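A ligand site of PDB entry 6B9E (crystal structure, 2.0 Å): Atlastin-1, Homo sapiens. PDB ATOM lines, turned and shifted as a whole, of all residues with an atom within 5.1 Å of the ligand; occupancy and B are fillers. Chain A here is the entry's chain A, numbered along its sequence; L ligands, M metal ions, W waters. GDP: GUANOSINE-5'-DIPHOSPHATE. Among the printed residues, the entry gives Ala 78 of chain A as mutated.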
ATOM      1  N   ALA A  76      23.006  12.400  -2.665  1.00  0.00           N
ATOM      2  CA  ALA A  76      23.784  12.581  -1.439  1.00  0.00           C
ATOM      3  C   ALA A  76      23.095  13.565  -0.475  1.00  0.00           C
ATOM      4  O   ALA A  76      22.273  14.410  -0.863  1.00  0.00           O
ATOM      5  CB  ALA A  76      25.193  13.056  -1.764  1.00  0.00           C
ATOM      6  N   PHE A  77      23.440  13.413   0.803  1.00  0.00           N
ATOM      7  CA  PHE A  77      22.861  14.189   1.887  1.00  0.00           C
ATOM      8  C   PHE A  77      23.319  15.654   1.835  1.00  0.00           C
ATOM      9  O   PHE A  77      24.415  15.979   1.369  1.00  0.00           O
ATOM     10  CB  PHE A  77      23.241  13.557   3.229  1.00  0.00           C
ATOM     11  CG  PHE A  77      23.271  14.519   4.396  1.00  0.00           C
ATOM     12  CD1 PHE A  77      22.093  14.898   5.029  1.00  0.00           C
ATOM     13  CD2 PHE A  77      24.473  15.021   4.869  1.00  0.00           C
ATOM     14  CE1 PHE A  77      22.122  15.776   6.108  1.00  0.00           C
ATOM     15  CE2 PHE A  77      24.508  15.910   5.941  1.00  0.00           C
ATOM     16  CZ  PHE A  77      23.333  16.287   6.560  1.00  0.00           C
ATOM     17  N   ALA A  78      22.431  16.550   2.300  1.00  0.00           N
ATOM     18  CA  ALA A  78      22.734  17.967   2.513  1.00  0.00           C
ATOM     19  C   ALA A  78      22.958  18.721   1.207  1.00  0.00           C
ATOM     20  O   ALA A  78      23.643  19.740   1.190  1.00  0.00           O
ATOM     21  CB  ALA A  78      23.940  18.167   3.439  1.00  0.00           C
ATOM     22  N   LYS A  79      22.379  18.227   0.112  1.00  0.00           N
ATOM     23  CA  LYS A  79      22.542  18.879  -1.177  1.00  0.00           C
ATOM     24  C   LYS A  79      21.257  19.559  -1.634  1.00  0.00           C
ATOM     25  O   LYS A  79      21.152  19.939  -2.808  1.00  0.00           O
ATOM     26  CB  LYS A  79      23.006  17.840  -2.208  1.00  0.00           C
ATOM     27  CG  LYS A  79      24.176  17.030  -1.726  1.00  0.00           C
ATOM     28  CD  LYS A  79      24.952  16.432  -2.860  1.00  0.00           C
ATOM     29  CE  LYS A  79      26.409  16.223  -2.442  1.00  0.00           C
ATOM     30  N   GLY A  80      20.294  19.754  -0.738  1.00  0.00           N
ATOM     31  CA  GLY A  80      19.132  20.557  -1.061  1.00  0.00           C
ATOM     32  C   GLY A  80      17.934  19.785  -1.585  1.00  0.00           C
ATOM     33  O   GLY A  80      17.109  20.388  -2.270  1.00  0.00           O
ATOM     34  N   LYS A  81      17.839  18.484  -1.307  1.00  0.00           N
ATOM     35  CA  LYS A  81      16.704  17.689  -1.777  1.00  0.00           C
ATOM     36  C   LYS A  81      15.391  18.171  -1.155  1.00  0.00           C
ATOM     37  O   LYS A  81      14.434  18.517  -1.869  1.00  0.00           O
ATOM     38  CB  LYS A  81      16.940  16.212  -1.468  1.00  0.00           C
ATOM     39  CG  LYS A  81      18.203  15.642  -2.129  1.00  0.00           C
ATOM     40  CD  LYS A  81      18.217  14.138  -2.125  1.00  0.00           C
ATOM     41  CE  LYS A  81      18.620  13.649  -0.758  1.00  0.00           C
ATOM     42  NZ  LYS A  81      19.794  14.452  -0.268  1.00  0.00           N
ATOM     43  N   SER A  82      15.326  18.236   0.171  1.00  0.00           N
ATOM     44  CA  SER A  82      14.086  18.664   0.821  1.00  0.00           C
ATOM     45  C   SER A  82      13.725  20.090   0.445  1.00  0.00           C
ATOM     46  O   SER A  82      12.543  20.415   0.243  1.00  0.00           O
ATOM     47  CB  SER A  82      14.190  18.503   2.327  1.00  0.00           C
ATOM     48  OG  SER A  82      14.453  17.145   2.641  1.00  0.00           O
ATOM     49  N   PHE A  83      14.722  20.986   0.389  1.00  0.00           N
ATOM     50  CA  PHE A  83      14.505  22.357  -0.070  1.00  0.00           C
ATOM     51  C   PHE A  83      13.774  22.388  -1.407  1.00  0.00           C
ATOM     52  O   PHE A  83      12.720  23.013  -1.547  1.00  0.00           O
ATOM     53  CB  PHE A  83      15.877  23.036  -0.166  1.00  0.00           C
ATOM     54  CG  PHE A  83      15.839  24.492  -0.508  1.00  0.00           C
ATOM     55  CD1 PHE A  83      15.588  25.444   0.474  1.00  0.00           C
ATOM     56  CD2 PHE A  83      16.148  24.915  -1.792  1.00  0.00           C
ATOM     57  CE1 PHE A  83      15.612  26.800   0.168  1.00  0.00           C
ATOM     58  CE2 PHE A  83      16.178  26.282  -2.105  1.00  0.00           C
ATOM     59  CZ  PHE A  83      15.901  27.220  -1.126  1.00  0.00           C
ATOM     60  N   SER A 112      11.252  18.531   6.189  1.00  0.00           N
ATOM     61  CA  SER A 112      12.268  19.217   6.983  1.00  0.00           C
ATOM     62  C   SER A 112      13.515  19.440   6.117  1.00  0.00           C
ATOM     63  O   SER A 112      13.939  18.532   5.388  1.00  0.00           O
ATOM     64  CB  SER A 112      12.596  18.391   8.219  1.00  0.00           C
ATOM     65  OG  SER A 112      13.679  18.950   8.937  1.00  0.00           O
ATOM     66  N   TRP A 113      14.050  20.665   6.131  1.00  0.00           N
ATOM     67  CA  TRP A 113      15.223  21.010   5.326  1.00  0.00           C
ATOM     68  C   TRP A 113      16.276  21.807   6.077  1.00  0.00           C
ATOM     69  O   TRP A 113      17.262  22.222   5.455  1.00  0.00           O
ATOM     70  CB  TRP A 113      14.799  21.790   4.056  1.00  0.00           C
ATOM     71  CG  TRP A 113      14.188  23.145   4.341  1.00  0.00           C
ATOM     72  CD1 TRP A 113      12.873  23.409   4.643  1.00  0.00           C
ATOM     73  CD2 TRP A 113      14.865  24.422   4.367  1.00  0.00           C
ATOM     74  NE1 TRP A 113      12.700  24.753   4.859  1.00  0.00           N
ATOM     75  CE2 TRP A 113      13.904  25.399   4.696  1.00  0.00           C
ATOM     76  CE3 TRP A 113      16.186  24.824   4.140  1.00  0.00           C
ATOM     77  CZ2 TRP A 113      14.217  26.759   4.798  1.00  0.00           C
ATOM     78  CZ3 TRP A 113      16.508  26.166   4.252  1.00  0.00           C
ATOM     79  CH2 TRP A 113      15.526  27.121   4.572  1.00  0.00           C
ATOM     80  N   ARG A 114      16.096  22.049   7.377  1.00  0.00           N
ATOM     81  CA  ARG A 114      17.012  22.796   8.246  1.00  0.00           C
ATOM     82  C   ARG A 114      17.009  24.289   7.922  1.00  0.00           C
ATOM     83  O   ARG A 114      16.040  24.997   8.205  1.00  0.00           O
ATOM     84  CB  ARG A 114      18.445  22.239   8.176  1.00  0.00           C
ATOM     85  N   ASP A 147      10.618  11.848  -0.447  1.00  0.00           N
ATOM     86  CA  ASP A 147      11.899  12.474  -0.133  1.00  0.00           C
ATOM     87  C   ASP A 147      12.817  11.377   0.397  1.00  0.00           C
ATOM     88  O   ASP A 147      12.516  10.747   1.420  1.00  0.00           O
ATOM     89  CB  ASP A 147      11.729  13.609   0.874  1.00  0.00           C
ATOM     90  CG  ASP A 147      13.011  14.401   1.095  1.00  0.00           C
ATOM     91  OD1 ASP A 147      14.058  14.097   0.453  1.00  0.00           O
ATOM     92  OD2 ASP A 147      12.945  15.353   1.883  1.00  0.00           O
ATOM     93  N   GLN A 149      16.265  10.149   1.676  1.00  0.00           N
ATOM     94  CA  GLN A 149      17.449  10.608   2.392  1.00  0.00           C
ATOM     95  C   GLN A 149      18.362   9.436   2.739  1.00  0.00           C
ATOM     96  O   GLN A 149      17.928   8.468   3.364  1.00  0.00           O
ATOM     97  CB  GLN A 149      17.060  11.370   3.656  1.00  0.00           C
ATOM     98  CG  GLN A 149      18.255  11.996   4.380  1.00  0.00           C
ATOM     99  CD  GLN A 149      18.911  13.123   3.580  1.00  0.00           C
ATOM    100  OE1 GLN A 149      19.513  12.888   2.537  1.00  0.00           O
ATOM    101  NE2 GLN A 149      18.765  14.356   4.063  1.00  0.00           N
ATOM    102  N   ASN A 178      19.741  14.142  -7.629  1.00  0.00           N
ATOM    103  CA  ASN A 178      20.248  15.442  -7.165  1.00  0.00           C
ATOM    104  C   ASN A 178      21.761  15.359  -7.002  1.00  0.00           C
ATOM    105  O   ASN A 178      22.246  14.570  -6.181  1.00  0.00           O
ATOM    106  CB  ASN A 178      19.595  15.832  -5.837  1.00  0.00           C
ATOM    107  CG  ASN A 178      19.798  17.314  -5.470  1.00  0.00           C
ATOM    108  OD1 ASN A 178      19.337  18.201  -6.185  1.00  0.00           O
ATOM    109  ND2 ASN A 178      20.383  17.570  -4.312  1.00  0.00           N
ATOM    110  N   ARG A 218      23.011  20.720  -9.144  1.00  0.00           N
ATOM    111  CA  ARG A 218      22.913  21.916  -8.329  1.00  0.00           C
ATOM    112  C   ARG A 218      24.242  22.683  -8.372  1.00  0.00           C
ATOM    113  O   ARG A 218      25.308  22.082  -8.525  1.00  0.00           O
ATOM    114  CB  ARG A 218      22.593  21.534  -6.870  1.00  0.00           C
ATOM    115  CG  ARG A 218      21.289  20.745  -6.657  1.00  0.00           C
ATOM    116  CD  ARG A 218      20.122  21.593  -7.048  1.00  0.00           C
ATOM    117  NE  ARG A 218      19.621  22.337  -5.907  1.00  0.00           N
ATOM    118  CZ  ARG A 218      18.861  21.827  -4.945  1.00  0.00           C
ATOM    119  NH1 ARG A 218      18.428  20.576  -5.021  1.00  0.00           N
ATOM    120  NH2 ARG A 218      18.499  22.619  -3.936  1.00  0.00           N
ATOM    121  N   ASP A 219      24.175  24.007  -8.189  1.00  0.00           N
ATOM    122  CA  ASP A 219      25.370  24.870  -8.122  1.00  0.00           C
ATOM    123  C   ASP A 219      26.261  24.691  -9.345  1.00  0.00           C
ATOM    124  O   ASP A 219      27.479  24.504  -9.215  1.00  0.00           O
ATOM    125  CB  ASP A 219      26.202  24.603  -6.851  1.00  0.00           C
ATOM    126  CG  ASP A 219      25.459  24.834  -5.579  1.00  0.00           C
ATOM    127  OD1 ASP A 219      24.307  25.323  -5.627  1.00  0.00           O
ATOM    128  OD2 ASP A 219      26.042  24.547  -4.509  1.00  0.00           O
ATOM    129  N   PRO A 271      21.603  27.078 -11.101  1.00  0.00           N
ATOM    130  CA  PRO A 271      22.638  27.919 -10.491  1.00  0.00           C
ATOM    131  C   PRO A 271      22.672  27.779  -8.975  1.00  0.00           C
ATOM    132  O   PRO A 271      21.750  27.246  -8.344  1.00  0.00           O
ATOM    133  CB  PRO A 271      22.246  29.348 -10.907  1.00  0.00           C
ATOM    134  CG  PRO A 271      20.854  29.286 -11.316  1.00  0.00           C
ATOM    135  CD  PRO A 271      20.522  27.861 -11.719  1.00  0.00           C
ATOM    136  N   HIS A 272      23.792  28.223  -8.418  1.00  0.00           N
ATOM    137  CA  HIS A 272      23.951  28.443  -6.987  1.00  0.00           C
ATOM    138  C   HIS A 272      22.808  29.332  -6.467  1.00  0.00           C
ATOM    139  O   HIS A 272      22.400  30.284  -7.148  1.00  0.00           O
ATOM    140  CB  HIS A 272      25.281  29.138  -6.726  1.00  0.00           C
ATOM    141  CG  HIS A 272      25.720  29.159  -5.292  1.00  0.00           C
ATOM    142  ND1 HIS A 272      26.568  28.211  -4.759  1.00  0.00           N
ATOM    143  CD2 HIS A 272      25.410  30.003  -4.285  1.00  0.00           C
ATOM    144  CE1 HIS A 272      26.790  28.500  -3.486  1.00  0.00           C
ATOM    145  NE2 HIS A 272      26.097  29.575  -3.171  1.00  0.00           N
ATOM    146  N   PRO A 273      22.256  29.042  -5.283  1.00  0.00           N
ATOM    147  CA  PRO A 273      21.109  29.819  -4.794  1.00  0.00           C
ATOM    148  C   PRO A 273      21.494  31.119  -4.090  1.00  0.00           C
ATOM    149  O   PRO A 273      20.604  31.828  -3.623  1.00  0.00           O
ATOM    150  CB  PRO A 273      20.440  28.844  -3.824  1.00  0.00           C
ATOM    151  CG  PRO A 273      21.605  28.066  -3.265  1.00  0.00           C
ATOM    152  CD  PRO A 273      22.539  27.878  -4.417  1.00  0.00           C
ATOM    153  N   VAL A 277      21.215  31.429   1.080  1.00  0.00           N
ATOM    154  CA  VAL A 277      20.717  30.059   1.035  1.00  0.00           C
ATOM    155  C   VAL A 277      21.824  29.078   1.380  1.00  0.00           C
ATOM    156  O   VAL A 277      21.559  27.961   1.846  1.00  0.00           O
ATOM    157  CB  VAL A 277      20.119  29.751  -0.351  1.00  0.00           C
ATOM    158  CG1 VAL A 277      19.475  28.365  -0.353  1.00  0.00           C
ATOM    159  CG2 VAL A 277      19.127  30.826  -0.748  1.00  0.00           C
ATOM    160  N   ALA A 278      23.071  29.458   1.107  1.00  0.00           N
ATOM    161  CA  ALA A 278      24.176  28.538   1.306  1.00  0.00           C
ATOM    162  C   ALA A 278      24.666  28.523   2.749  1.00  0.00           C
ATOM    163  O   ALA A 278      24.878  27.454   3.320  1.00  0.00           O
ATOM    164  CB  ALA A 278      25.316  28.894   0.352  1.00  0.00           C
ATOM    165  N   PHE A 283      18.287  31.870   7.910  1.00  0.00           N
ATOM    166  CA  PHE A 283      17.588  31.851   6.630  1.00  0.00           C
ATOM    167  C   PHE A 283      16.444  30.846   6.684  1.00  0.00           C
ATOM    168  O   PHE A 283      16.667  29.655   6.956  1.00  0.00           O
ATOM    169  CB  PHE A 283      18.565  31.513   5.506  1.00  0.00           C
ATOM    170  CG  PHE A 283      17.909  31.099   4.224  1.00  0.00           C
ATOM    171  CD1 PHE A 283      17.310  32.036   3.392  1.00  0.00           C
ATOM    172  CD2 PHE A 283      17.905  29.784   3.836  1.00  0.00           C
ATOM    173  CE1 PHE A 283      16.714  31.658   2.210  1.00  0.00           C
ATOM    174  CE2 PHE A 283      17.295  29.390   2.646  1.00  0.00           C
ATOM    175  CZ  PHE A 283      16.705  30.326   1.837  1.00  0.00           C
ATOM    176  N   PHE A 294      18.667  31.909  -9.614  1.00  0.00           N
ATOM    177  CA  PHE A 294      18.202  30.609  -9.127  1.00  0.00           C
ATOM    178  C   PHE A 294      16.672  30.534  -9.198  1.00  0.00           C
ATOM    179  O   PHE A 294      16.113  29.515  -9.642  1.00  0.00           O
ATOM    180  CB  PHE A 294      18.714  30.370  -7.706  1.00  0.00           C
ATOM    181  CG  PHE A 294      18.164  29.103  -7.054  1.00  0.00           C
ATOM    182  CD1 PHE A 294      16.956  29.120  -6.351  1.00  0.00           C
ATOM    183  CD2 PHE A 294      18.864  27.894  -7.125  1.00  0.00           C
ATOM    184  CE1 PHE A 294      16.458  27.979  -5.747  1.00  0.00           C
ATOM    185  CE2 PHE A 294      18.375  26.757  -6.521  1.00  0.00           C
ATOM    186  CZ  PHE A 294      17.158  26.793  -5.827  1.00  0.00           C
HETATM  187  PB  GDP L   1      19.047  17.418   1.707  1.00  0.00           P
HETATM  188  O1B GDP L   1      19.691  16.718   2.885  1.00  0.00           O
HETATM  189  O2B GDP L   1      17.541  17.181   1.777  1.00  0.00           O
HETATM  190  O3B GDP L   1      19.611  16.842   0.432  1.00  0.00           O
HETATM  191  O3A GDP L   1      19.359  18.973   1.700  1.00  0.00           O
HETATM  192  PA  GDP L   1      18.456  20.027   2.521  1.00  0.00           P
HETATM  193  O1A GDP L   1      18.138  19.508   3.916  1.00  0.00           O
HETATM  194  O2A GDP L   1      17.224  20.352   1.716  1.00  0.00           O
HETATM  195  O5' GDP L   1      19.432  21.329   2.520  1.00  0.00           O
HETATM  196  C5' GDP L   1      20.359  21.678   3.560  1.00  0.00           C
HETATM  197  C4' GDP L   1      20.978  23.047   3.287  1.00  0.00           C
HETATM  198  O4' GDP L   1      21.291  23.193   1.895  1.00  0.00           O
HETATM  199  C3' GDP L   1      20.059  24.222   3.612  1.00  0.00           C
HETATM  200  O3' GDP L   1      20.813  25.228   4.286  1.00  0.00           O
HETATM  201  C2' GDP L   1      19.659  24.804   2.277  1.00  0.00           C
HETATM  202  O2' GDP L   1      19.422  26.211   2.366  1.00  0.00           O
HETATM  203  C1' GDP L   1      20.908  24.504   1.465  1.00  0.00           C
HETATM  204  N9  GDP L   1      20.638  24.513   0.020  1.00  0.00           N
HETATM  205  C8  GDP L   1      19.448  24.361  -0.605  1.00  0.00           C
HETATM  206  N7  GDP L   1      19.593  24.407  -1.960  1.00  0.00           N
HETATM  207  C5  GDP L   1      20.912  24.587  -2.212  1.00  0.00           C
HETATM  208  C6  GDP L   1      21.771  24.716  -3.412  1.00  0.00           C
HETATM  209  O6  GDP L   1      21.260  24.677  -4.555  1.00  0.00           O
HETATM  210  N1  GDP L   1      23.097  24.908  -3.220  1.00  0.00           N
HETATM  211  C2  GDP L   1      23.672  24.958  -1.997  1.00  0.00           C
HETATM  212  N2  GDP L   1      25.018  25.133  -1.901  1.00  0.00           N
HETATM  213  N3  GDP L   1      22.943  24.834  -0.856  1.00  0.00           N
HETATM  214  C4  GDP L   1      21.592  24.656  -0.902  1.00  0.00           C
HETATM  215 MG    MG M   1      16.145  14.711   2.237  1.00  0.00          MG
HETATM  216  O   HOH W   1      23.327  21.684  -3.149  1.00  0.00           O
HETATM  217  O   HOH W   2      21.452  24.780  -7.166  1.00  0.00           O
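The backbone carbonyl oxygen (O) of Trp 113 lies close to an oxygen (O1A) of the ligand (3.2 Å).
Residues that only touch the ligand: Pro 273, Phe 77, Ala 76 and Phe 283.
Within 4 Å of the ligand: Ala 76, Phe 77, Ala 78, Lys 79, Gly 80, Lys 81, Ser 82, Phe 83, Trp 113, Gln 149, Arg 218, Asp 219, Pro 273, Val 277 and Phe 283.
Water W2 lies within hydrogen-bond range of an oxygen (O6) of the ligand, the backbone carbonyl oxygen of Pro 271, the backbone NH of Asp 219 and the guanidinium group of Arg 218.
Water W1 lies within hydrogen-bond range of O of Lys 79 (2.8 Å) and N1 of the ligand (3.2 Å).
O of Ala 76 lies within hydrogen-bond range of NZ of Lys 81 (2.5 Å).
The backbone carbonyl oxygen of Lys 79 lies within hydrogen-bond range of the side-chain amide nitrogen of Asn 178 (2.9 Å).
OG of Ser 82 lies within hydrogen-bond range of OD2 of Asp 147 (2.5 Å).
O of Ser 112 lies close to OG of Ser 82.
The guanidinium group of Arg 218 sits at hydrogen-bond distance from the side-chain amide oxygen of Asn 178, 2.8 Å away.
The side-chain amino group of Lys 81 is in hydrogen-bond range of the side-chain amide oxygen of Gln 149 (3.2 Å).
The backbone carbonyl oxygen (O) of Gly 80 lies within hydrogen-bond range of the guanidinium group (NH1) of Arg 218, at 3.1 Å.
An oxygen (O2') of the ligand sits at hydrogen-bond distance from the backbone carbonyl oxygen of Val 277, at 2.8 Å.
The guanidinium group (NH2) of Arg 218 is in hydrogen-bond range of a nitrogen (N7) of the ligand (2.9 Å).
The backbone NH (N) of Phe 83 lies within hydrogen-bond range of an oxygen (O2A) of the ligand (2.9 Å).
An oxygen (O1B) of the ligand sits at hydrogen-bond distance from the backbone NH of Ala 78 (2.8 Å).
NE2 of Gln 149 is in hydrogen-bond range of O1B of the ligand, 2.8 Å away.
The side-chain amino group (NZ) of Lys 81 is in salt-bridge range of an oxygen (O3B) of the ligand (2.5 Å).
O2B of the ligand lies within hydrogen-bond range of N of Ser 82, 2.9 Å away.
OD1 of Asp 219 sits at hydrogen-bond distance from N1 of the ligand, 2.7 Å away.
O3B of the ligand is in hydrogen-bond range of N of Lys 81 (3.0 Å).
The backbone NH (N) of Gly 80 is in hydrogen-bond range of an oxygen (O3A) of the ligand, at 2.7 Å.
O3B of the ligand lies within hydrogen-bond range of N of Lys 79, at 3.1 Å.
OG of Ser 82 lies within hydrogen-bond range of O2B of the ligand (3.2 Å).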
